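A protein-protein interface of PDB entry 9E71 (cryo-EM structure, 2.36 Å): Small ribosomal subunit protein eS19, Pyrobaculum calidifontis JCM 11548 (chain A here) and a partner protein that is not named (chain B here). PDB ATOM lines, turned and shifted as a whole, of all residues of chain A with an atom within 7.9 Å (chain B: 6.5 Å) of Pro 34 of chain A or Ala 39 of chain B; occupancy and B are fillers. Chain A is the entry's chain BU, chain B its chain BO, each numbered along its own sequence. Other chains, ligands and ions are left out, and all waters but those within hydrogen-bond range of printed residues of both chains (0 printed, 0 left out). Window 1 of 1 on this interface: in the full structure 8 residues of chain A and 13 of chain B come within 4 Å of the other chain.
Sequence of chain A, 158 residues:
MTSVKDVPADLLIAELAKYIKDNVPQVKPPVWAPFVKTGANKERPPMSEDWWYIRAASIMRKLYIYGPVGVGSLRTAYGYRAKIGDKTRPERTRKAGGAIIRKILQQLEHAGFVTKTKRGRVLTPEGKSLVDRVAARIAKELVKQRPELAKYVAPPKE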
ATOM      1  N   PRO A  29      16.360 -26.546 -38.474  1.00  0.00           N
ATOM      2  CA  PRO A  29      16.952 -27.268 -37.343  1.00  0.00           C
ATOM      3  C   PRO A  29      16.611 -28.745 -37.396  1.00  0.00           C
ATOM      4  O   PRO A  29      15.489 -29.121 -37.765  1.00  0.00           O
ATOM      5  CB  PRO A  29      16.314 -26.605 -36.114  1.00  0.00           C
ATOM      6  CG  PRO A  29      15.559 -25.429 -36.603  1.00  0.00           C
ATOM      7  CD  PRO A  29      15.709 -25.292 -38.072  1.00  0.00           C
ATOM      8  N   PRO A  30      17.547 -29.613 -37.037  1.00  0.00           N
ATOM      9  CA  PRO A  30      17.277 -31.049 -37.046  1.00  0.00           C
ATOM     10  C   PRO A  30      16.589 -31.487 -35.759  1.00  0.00           C
ATOM     11  O   PRO A  30      16.460 -30.732 -34.795  1.00  0.00           O
ATOM     12  CB  PRO A  30      18.669 -31.673 -37.173  1.00  0.00           C
ATOM     13  CG  PRO A  30      19.644 -30.587 -36.815  1.00  0.00           C
ATOM     14  CD  PRO A  30      18.902 -29.314 -36.557  1.00  0.00           C
ATOM     15  N   VAL A  31      16.171 -32.754 -35.756  1.00  0.00           N
ATOM     16  CA  VAL A  31      15.344 -33.287 -34.680  1.00  0.00           C
ATOM     17  C   VAL A  31      16.079 -33.348 -33.348  1.00  0.00           C
ATOM     18  O   VAL A  31      15.438 -33.412 -32.295  1.00  0.00           O
ATOM     19  CB  VAL A  31      14.814 -34.679 -35.073  1.00  0.00           C
ATOM     20  CG1 VAL A  31      15.821 -35.752 -34.712  1.00  0.00           C
ATOM     21  CG2 VAL A  31      13.481 -34.945 -34.409  1.00  0.00           C
ATOM     22  N   TRP A  32      17.408 -33.344 -33.361  1.00  0.00           N
ATOM     23  CA  TRP A  32      18.183 -33.337 -32.131  1.00  0.00           C
ATOM     24  C   TRP A  32      18.562 -31.938 -31.678  1.00  0.00           C
ATOM     25  O   TRP A  32      19.328 -31.804 -30.719  1.00  0.00           O
ATOM     26  CB  TRP A  32      19.449 -34.183 -32.287  1.00  0.00           C
ATOM     27  CG  TRP A  32      20.233 -33.954 -33.546  1.00  0.00           C
ATOM     28  CD1 TRP A  32      20.200 -34.714 -34.672  1.00  0.00           C
ATOM     29  CD2 TRP A  32      21.188 -32.915 -33.794  1.00  0.00           C
ATOM     30  NE1 TRP A  32      21.062 -34.211 -35.610  1.00  0.00           N
ATOM     31  CE2 TRP A  32      21.683 -33.107 -35.096  1.00  0.00           C
ATOM     32  CE3 TRP A  32      21.669 -31.839 -33.042  1.00  0.00           C
ATOM     33  CZ2 TRP A  32      22.631 -32.266 -35.665  1.00  0.00           C
ATOM     34  CZ3 TRP A  32      22.611 -31.005 -33.608  1.00  0.00           C
ATOM     35  CH2 TRP A  32      23.082 -31.222 -34.907  1.00  0.00           C
ATOM     36  N   ALA A  33      18.062 -30.905 -32.349  1.00  0.00           N
ATOM     37  CA  ALA A  33      18.379 -29.529 -31.972  1.00  0.00           C
ATOM     38  C   ALA A  33      17.998 -29.150 -30.542  1.00  0.00           C
ATOM     39  O   ALA A  33      18.844 -28.552 -29.856  1.00  0.00           O
ATOM     40  CB  ALA A  33      17.717 -28.566 -32.965  1.00  0.00           C
ATOM     41  N   PRO A  34      16.788 -29.427 -30.036  1.00  0.00           N
ATOM     42  CA  PRO A  34      16.468 -29.021 -28.653  1.00  0.00           C
ATOM     43  C   PRO A  34      17.286 -29.712 -27.572  1.00  0.00           C
ATOM     44  O   PRO A  34      17.328 -29.198 -26.450  1.00  0.00           O
ATOM     45  CB  PRO A  34      14.981 -29.370 -28.502  1.00  0.00           C
ATOM     46  CG  PRO A  34      14.510 -29.853 -29.784  1.00  0.00           C
ATOM     47  CD  PRO A  34      15.603 -29.908 -30.769  1.00  0.00           C
ATOM     48  N   PHE A  35      17.929 -30.842 -27.851  1.00  0.00           N
ATOM     49  CA  PHE A  35      18.543 -31.656 -26.810  1.00  0.00           C
ATOM     50  C   PHE A  35      20.050 -31.473 -26.695  1.00  0.00           C
ATOM     51  O   PHE A  35      20.694 -32.224 -25.957  1.00  0.00           O
ATOM     52  CB  PHE A  35      18.236 -33.134 -27.052  1.00  0.00           C
ATOM     53  CG  PHE A  35      16.777 -33.440 -27.152  1.00  0.00           C
ATOM     54  CD1 PHE A  35      15.988 -33.464 -26.026  1.00  0.00           C
ATOM     55  CD2 PHE A  35      16.195 -33.700 -28.375  1.00  0.00           C
ATOM     56  CE1 PHE A  35      14.648 -33.739 -26.115  1.00  0.00           C
ATOM     57  CE2 PHE A  35      14.856 -33.978 -28.469  1.00  0.00           C
ATOM     58  CZ  PHE A  35      14.083 -33.998 -27.337  1.00  0.00           C
ATOM     59  N   VAL A  36      20.641 -30.507 -27.396  1.00  0.00           N
ATOM     60  CA  VAL A  36      22.093 -30.421 -27.467  1.00  0.00           C
ATOM     61  C   VAL A  36      22.554 -28.999 -27.194  1.00  0.00           C
ATOM     62  O   VAL A  36      21.789 -28.036 -27.291  1.00  0.00           O
ATOM     63  CB  VAL A  36      22.643 -30.898 -28.831  1.00  0.00           C
ATOM     64  CG1 VAL A  36      22.273 -32.345 -29.076  1.00  0.00           C
ATOM     65  CG2 VAL A  36      22.134 -30.016 -29.951  1.00  0.00           C
ATOM     66  N   LYS A  37      23.828 -28.886 -26.839  1.00  0.00           N
ATOM     67  CA  LYS A  37      24.539 -27.623 -26.754  1.00  0.00           C
ATOM     68  C   LYS A  37      25.478 -27.499 -27.945  1.00  0.00           C
ATOM     69  O   LYS A  37      25.746 -28.467 -28.658  1.00  0.00           O
ATOM     70  CB  LYS A  37      25.325 -27.519 -25.444  1.00  0.00           C
ATOM     71  CG  LYS A  37      24.551 -27.935 -24.214  1.00  0.00           C
ATOM     72  CD  LYS A  37      25.477 -28.089 -23.032  1.00  0.00           C
ATOM     73  CE  LYS A  37      24.737 -28.555 -21.802  1.00  0.00           C
ATOM     74  NZ  LYS A  37      25.692 -29.016 -20.764  1.00  0.00           N
ATOM     75  N   PRO A  45      22.524 -24.997 -22.694  1.00  0.00           N
ATOM     76  CA  PRO A  45      22.217 -24.881 -24.116  1.00  0.00           C
ATOM     77  C   PRO A  45      21.944 -23.436 -24.483  1.00  0.00           C
ATOM     78  O   PRO A  45      21.745 -22.594 -23.595  1.00  0.00           O
ATOM     79  CB  PRO A  45      20.962 -25.748 -24.285  1.00  0.00           C
ATOM     80  CG  PRO A  45      20.373 -25.878 -22.932  1.00  0.00           C
ATOM     81  CD  PRO A  45      21.387 -25.498 -21.903  1.00  0.00           C
ATOM     82  N   PRO A  46      21.950 -23.106 -25.773  1.00  0.00           N
ATOM     83  CA  PRO A  46      21.684 -21.722 -26.180  1.00  0.00           C
ATOM     84  C   PRO A  46      20.262 -21.312 -25.834  1.00  0.00           C
ATOM     85  O   PRO A  46      19.331 -22.114 -25.906  1.00  0.00           O
ATOM     86  CB  PRO A  46      21.910 -21.736 -27.696  1.00  0.00           C
ATOM     87  CG  PRO A  46      22.319 -23.109 -28.061  1.00  0.00           C
ATOM     88  CD  PRO A  46      22.143 -24.017 -26.910  1.00  0.00           C
ATOM     89  N   TRP A  51      18.679 -19.894 -32.635  1.00  0.00           N
ATOM     90  CA  TRP A  51      20.130 -20.014 -32.598  1.00  0.00           C
ATOM     91  C   TRP A  51      20.664 -20.719 -33.833  1.00  0.00           C
ATOM     92  O   TRP A  51      21.771 -20.414 -34.282  1.00  0.00           O
ATOM     93  CB  TRP A  51      20.580 -20.734 -31.324  1.00  0.00           C
ATOM     94  CG  TRP A  51      20.154 -22.159 -31.211  1.00  0.00           C
ATOM     95  CD1 TRP A  51      19.017 -22.627 -30.629  1.00  0.00           C
ATOM     96  CD2 TRP A  51      20.869 -23.309 -31.672  1.00  0.00           C
ATOM     97  NE1 TRP A  51      18.971 -23.995 -30.709  1.00  0.00           N
ATOM     98  CE2 TRP A  51      20.098 -24.438 -31.346  1.00  0.00           C
ATOM     99  CE3 TRP A  51      22.082 -23.491 -32.339  1.00  0.00           C
ATOM    100  CZ2 TRP A  51      20.500 -25.729 -31.660  1.00  0.00           C
ATOM    101  CZ3 TRP A  51      22.477 -24.777 -32.653  1.00  0.00           C
ATOM    102  CH2 TRP A  51      21.689 -25.877 -32.314  1.00  0.00           C
ATOM    103  N   ILE B  34      18.994 -28.290 -15.877  1.00  0.00           N
ATOM    104  CA  ILE B  34      18.744 -27.174 -16.781  1.00  0.00           C
ATOM    105  C   ILE B  34      18.669 -27.655 -18.225  1.00  0.00           C
ATOM    106  O   ILE B  34      17.815 -27.201 -18.996  1.00  0.00           O
ATOM    107  CB  ILE B  34      19.810 -26.082 -16.595  1.00  0.00           C
ATOM    108  CG1 ILE B  34      19.223 -24.943 -15.772  1.00  0.00           C
ATOM    109  CG2 ILE B  34      20.293 -25.567 -17.935  1.00  0.00           C
ATOM    110  CD1 ILE B  34      17.898 -24.461 -16.300  1.00  0.00           C
ATOM    111  N   ALA B  35      19.554 -28.575 -18.613  1.00  0.00           N
ATOM    112  CA  ALA B  35      19.531 -29.105 -19.972  1.00  0.00           C
ATOM    113  C   ALA B  35      18.244 -29.874 -20.238  1.00  0.00           C
ATOM    114  O   ALA B  35      17.607 -29.704 -21.285  1.00  0.00           O
ATOM    115  CB  ALA B  35      20.749 -29.997 -20.205  1.00  0.00           C
ATOM    116  N   THR B  36      17.836 -30.709 -19.282  1.00  0.00           N
ATOM    117  CA  THR B  36      16.601 -31.470 -19.431  1.00  0.00           C
ATOM    118  C   THR B  36      15.383 -30.556 -19.457  1.00  0.00           C
ATOM    119  O   THR B  36      14.445 -30.790 -20.223  1.00  0.00           O
ATOM    120  CB  THR B  36      16.482 -32.496 -18.305  1.00  0.00           C
ATOM    121  OG1 THR B  36      17.282 -33.639 -18.616  1.00  0.00           O
ATOM    122  CG2 THR B  36      15.047 -32.935 -18.140  1.00  0.00           C
ATOM    123  N   ALA B  37      15.382 -29.504 -18.636  1.00  0.00           N
ATOM    124  CA  ALA B  37      14.259 -28.573 -18.628  1.00  0.00           C
ATOM    125  C   ALA B  37      14.157 -27.812 -19.941  1.00  0.00           C
ATOM    126  O   ALA B  37      13.057 -27.632 -20.480  1.00  0.00           O
ATOM    127  CB  ALA B  37      14.394 -27.605 -17.458  1.00  0.00           C
ATOM    128  N   TYR B  38      15.294 -27.353 -20.473  1.00  0.00           N
ATOM    129  CA  TYR B  38      15.291 -26.666 -21.761  1.00  0.00           C
ATOM    130  C   TYR B  38      14.826 -27.589 -22.878  1.00  0.00           C
ATOM    131  O   TYR B  38      14.067 -27.176 -23.764  1.00  0.00           O
ATOM    132  CB  TYR B  38      16.685 -26.132 -22.067  1.00  0.00           C
ATOM    133  CG  TYR B  38      16.869 -24.661 -21.816  1.00  0.00           C
ATOM    134  CD1 TYR B  38      16.307 -23.720 -22.658  1.00  0.00           C
ATOM    135  CD2 TYR B  38      17.629 -24.214 -20.749  1.00  0.00           C
ATOM    136  CE1 TYR B  38      16.484 -22.376 -22.439  1.00  0.00           C
ATOM    137  CE2 TYR B  38      17.812 -22.873 -20.524  1.00  0.00           C
ATOM    138  CZ  TYR B  38      17.239 -21.959 -21.372  1.00  0.00           C
ATOM    139  OH  TYR B  38      17.419 -20.617 -21.146  1.00  0.00           O
ATOM    140  N   ALA B  39      15.275 -28.845 -22.851  1.00  0.00           N
ATOM    141  CA  ALA B  39      14.842 -29.810 -23.851  1.00  0.00           C
ATOM    142  C   ALA B  39      13.345 -30.067 -23.762  1.00  0.00           C
ATOM    143  O   ALA B  39      12.664 -30.151 -24.788  1.00  0.00           O
ATOM    144  CB  ALA B  39      15.618 -31.111 -23.683  1.00  0.00           C
ATOM    145  N   ILE B  40      12.816 -30.190 -22.543  1.00  0.00           N
ATOM    146  CA  ILE B  40      11.387 -30.422 -22.351  1.00  0.00           C
ATOM    147  C   ILE B  40      10.579 -29.245 -22.877  1.00  0.00           C
ATOM    148  O   ILE B  40       9.563 -29.422 -23.558  1.00  0.00           O
ATOM    149  CB  ILE B  40      11.086 -30.685 -20.866  1.00  0.00           C
ATOM    150  CG1 ILE B  40      11.261 -32.165 -20.535  1.00  0.00           C
ATOM    151  CG2 ILE B  40       9.694 -30.209 -20.513  1.00  0.00           C
ATOM    152  CD1 ILE B  40      11.264 -32.452 -19.057  1.00  0.00           C
ATOM    153  N   CYS B  41      11.021 -28.023 -22.568  1.00  0.00           N
ATOM    154  CA  CYS B  41      10.304 -26.837 -23.023  1.00  0.00           C
ATOM    155  C   CYS B  41      10.320 -26.719 -24.541  1.00  0.00           C
ATOM    156  O   CYS B  41       9.286 -26.439 -25.157  1.00  0.00           O
ATOM    157  CB  CYS B  41      10.906 -25.589 -22.388  1.00  0.00           C
ATOM    158  SG  CYS B  41      10.719 -25.533 -20.609  1.00  0.00           S
ATOM    159  N   ARG B  42      11.478 -26.944 -25.167  1.00  0.00           N
ATOM    160  CA  ARG B  42      11.533 -26.831 -26.621  1.00  0.00           C
ATOM    161  C   ARG B  42      10.763 -27.951 -27.305  1.00  0.00           C
ATOM    162  O   ARG B  42      10.145 -27.723 -28.350  1.00  0.00           O
ATOM    163  CB  ARG B  42      12.984 -26.806 -27.098  1.00  0.00           C
ATOM    164  CG  ARG B  42      13.549 -25.404 -27.159  1.00  0.00           C
ATOM    165  CD  ARG B  42      14.988 -25.353 -26.702  1.00  0.00           C
ATOM    166  NE  ARG B  42      15.466 -23.979 -26.620  1.00  0.00           N
ATOM    167  CZ  ARG B  42      16.720 -23.635 -26.373  1.00  0.00           C
ATOM    168  NH1 ARG B  42      17.676 -24.543 -26.257  1.00  0.00           N
ATOM    169  NH2 ARG B  42      17.025 -22.349 -26.245  1.00  0.00           N
ATOM    170  N   LYS B  43      10.778 -29.158 -26.738  1.00  0.00           N
ATOM    171  CA  LYS B  43      10.029 -30.260 -27.329  1.00  0.00           C
ATOM    172  C   LYS B  43       8.528 -30.048 -27.202  1.00  0.00           C
ATOM    173  O   LYS B  43       7.773 -30.360 -28.129  1.00  0.00           O
ATOM    174  CB  LYS B  43      10.439 -31.575 -26.674  1.00  0.00           C
ATOM    175  CG  LYS B  43      10.207 -32.780 -27.549  1.00  0.00           C
ATOM    176  CD  LYS B  43      11.200 -32.814 -28.689  1.00  0.00           C
ATOM    177  CE  LYS B  43      11.029 -34.068 -29.514  1.00  0.00           C
ATOM    178  NZ  LYS B  43      10.043 -33.860 -30.603  1.00  0.00           N
ATOM    179  N   LEU B  44       8.072 -29.529 -26.064  1.00  0.00           N
ATOM    180  CA  LEU B  44       6.655 -29.300 -25.840  1.00  0.00           C
ATOM    181  C   LEU B  44       6.181 -27.965 -26.389  1.00  0.00           C
ATOM    182  O   LEU B  44       4.990 -27.655 -26.293  1.00  0.00           O
ATOM    183  CB  LEU B  44       6.340 -29.386 -24.347  1.00  0.00           C
ATOM    184  CG  LEU B  44       6.531 -30.745 -23.686  1.00  0.00           C
ATOM    185  CD1 LEU B  44       6.351 -30.637 -22.188  1.00  0.00           C
ATOM    186  CD2 LEU B  44       5.556 -31.743 -24.266  1.00  0.00           C
ATOM    187  N   LEU B  70       9.848 -38.372 -19.587  1.00  0.00           N
ATOM    188  CA  LEU B  70      10.805 -37.836 -20.551  1.00  0.00           C
ATOM    189  C   LEU B  70      11.395 -38.903 -21.465  1.00  0.00           C
ATOM    190  O   LEU B  70      11.841 -38.575 -22.568  1.00  0.00           O
ATOM    191  CB  LEU B  70      11.941 -37.110 -19.831  1.00  0.00           C
ATOM    192  CG  LEU B  70      12.978 -36.467 -20.755  1.00  0.00           C
ATOM    193  CD1 LEU B  70      12.447 -35.177 -21.336  1.00  0.00           C
ATOM    194  CD2 LEU B  70      14.295 -36.233 -20.046  1.00  0.00           C
ATOM    195  N   ALA B  74      12.800 -37.551 -25.237  1.00  0.00           N
ATOM    196  CA  ALA B  74      14.207 -37.342 -25.545  1.00  0.00           C
ATOM    197  C   ALA B  74      14.830 -38.610 -26.096  1.00  0.00           C
ATOM    198  O   ALA B  74      14.288 -39.708 -25.965  1.00  0.00           O
ATOM    199  CB  ALA B  74      14.943 -36.879 -24.294  1.00  0.00           C
ATOM    200  N   PHE B  78      20.027 -38.971 -23.622  1.00  0.00           N
ATOM    201  CA  PHE B  78      19.672 -37.788 -22.855  1.00  0.00           C
ATOM    202  C   PHE B  78      19.051 -38.128 -21.503  1.00  0.00           C
ATOM    203  O   PHE B  78      18.674 -37.218 -20.759  1.00  0.00           O
ATOM    204  CB  PHE B  78      18.720 -36.925 -23.685  1.00  0.00           C
ATOM    205  CG  PHE B  78      18.682 -35.486 -23.283  1.00  0.00           C
ATOM    206  CD1 PHE B  78      19.768 -34.664 -23.501  1.00  0.00           C
ATOM    207  CD2 PHE B  78      17.547 -34.948 -22.711  1.00  0.00           C
ATOM    208  CE1 PHE B  78      19.729 -33.336 -23.135  1.00  0.00           C
ATOM    209  CE2 PHE B  78      17.504 -33.624 -22.347  1.00  0.00           C
ATOM    210  CZ  PHE B  78      18.595 -32.817 -22.559  1.00  0.00           C
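Of the 14 printed residues of chain B, 6 touch a printed residue of chain A. Printed residues of chain B that touch a printed residue of chain A: Tyr 38, Ala 39, Arg 42, Lys 43, Ala 74 and Phe 78. Hydrophobic or aromatic side chains of chain A within 4 Å of the printed part of chain B: Pro 34, Phe 35 and Pro 45. Along chain A the printed residues that touch a printed residue of chain B span positions 34 to 46. Among the printed residues, no Asp or Glu carboxylate lies within 4 Å of a Lys or Arg side-chain nitrogen of the other chain.
The guanidinium group (NH1) of Arg 42 of chain B lies within hydrogen-bond range of the backbone carbonyl oxygen (O) of Pro 46 of chain A.
Of chain B, only Ala 39 and Arg 42 come within 4 Å of Pro 34 of chain A. Trp 51 of chain A touches none of the printed residues of chain B. Of the printed residues of chain A, Arg 42 of chain B touches Pro 34 (3.5 Å) and Pro 46 (2.3 Å). Of the printed residues of chain A, Ala 74 of chain B touches Phe 35. Of the printed residues of chain A, Phe 78 of chain B touches Phe 35 (3.2 Å). The nearest residue of chain B that does not touch Pro 34 of chain A is Lys 43 of chain B (4.6 Å). The nearest printed residue of chain B that does not touch Phe 35 of chain A is Ile 40 of chain B (5.4 Å).
Among the printed residues, merely in contact across the chains: Phe 35 of chain A with Phe 78 of chain B, Phe 35 of chain A with Ala 39 of chain B, Phe 35 of chain A with Lys 43 of chain B, Pro 34 of chain A with Arg 42 of chain B, Phe 35 of chain A with Ala 74 of chain B, Pro 34 of chain A with Ala 39 of chain B and Pro 45 of chain A with Tyr 38 of chain B.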
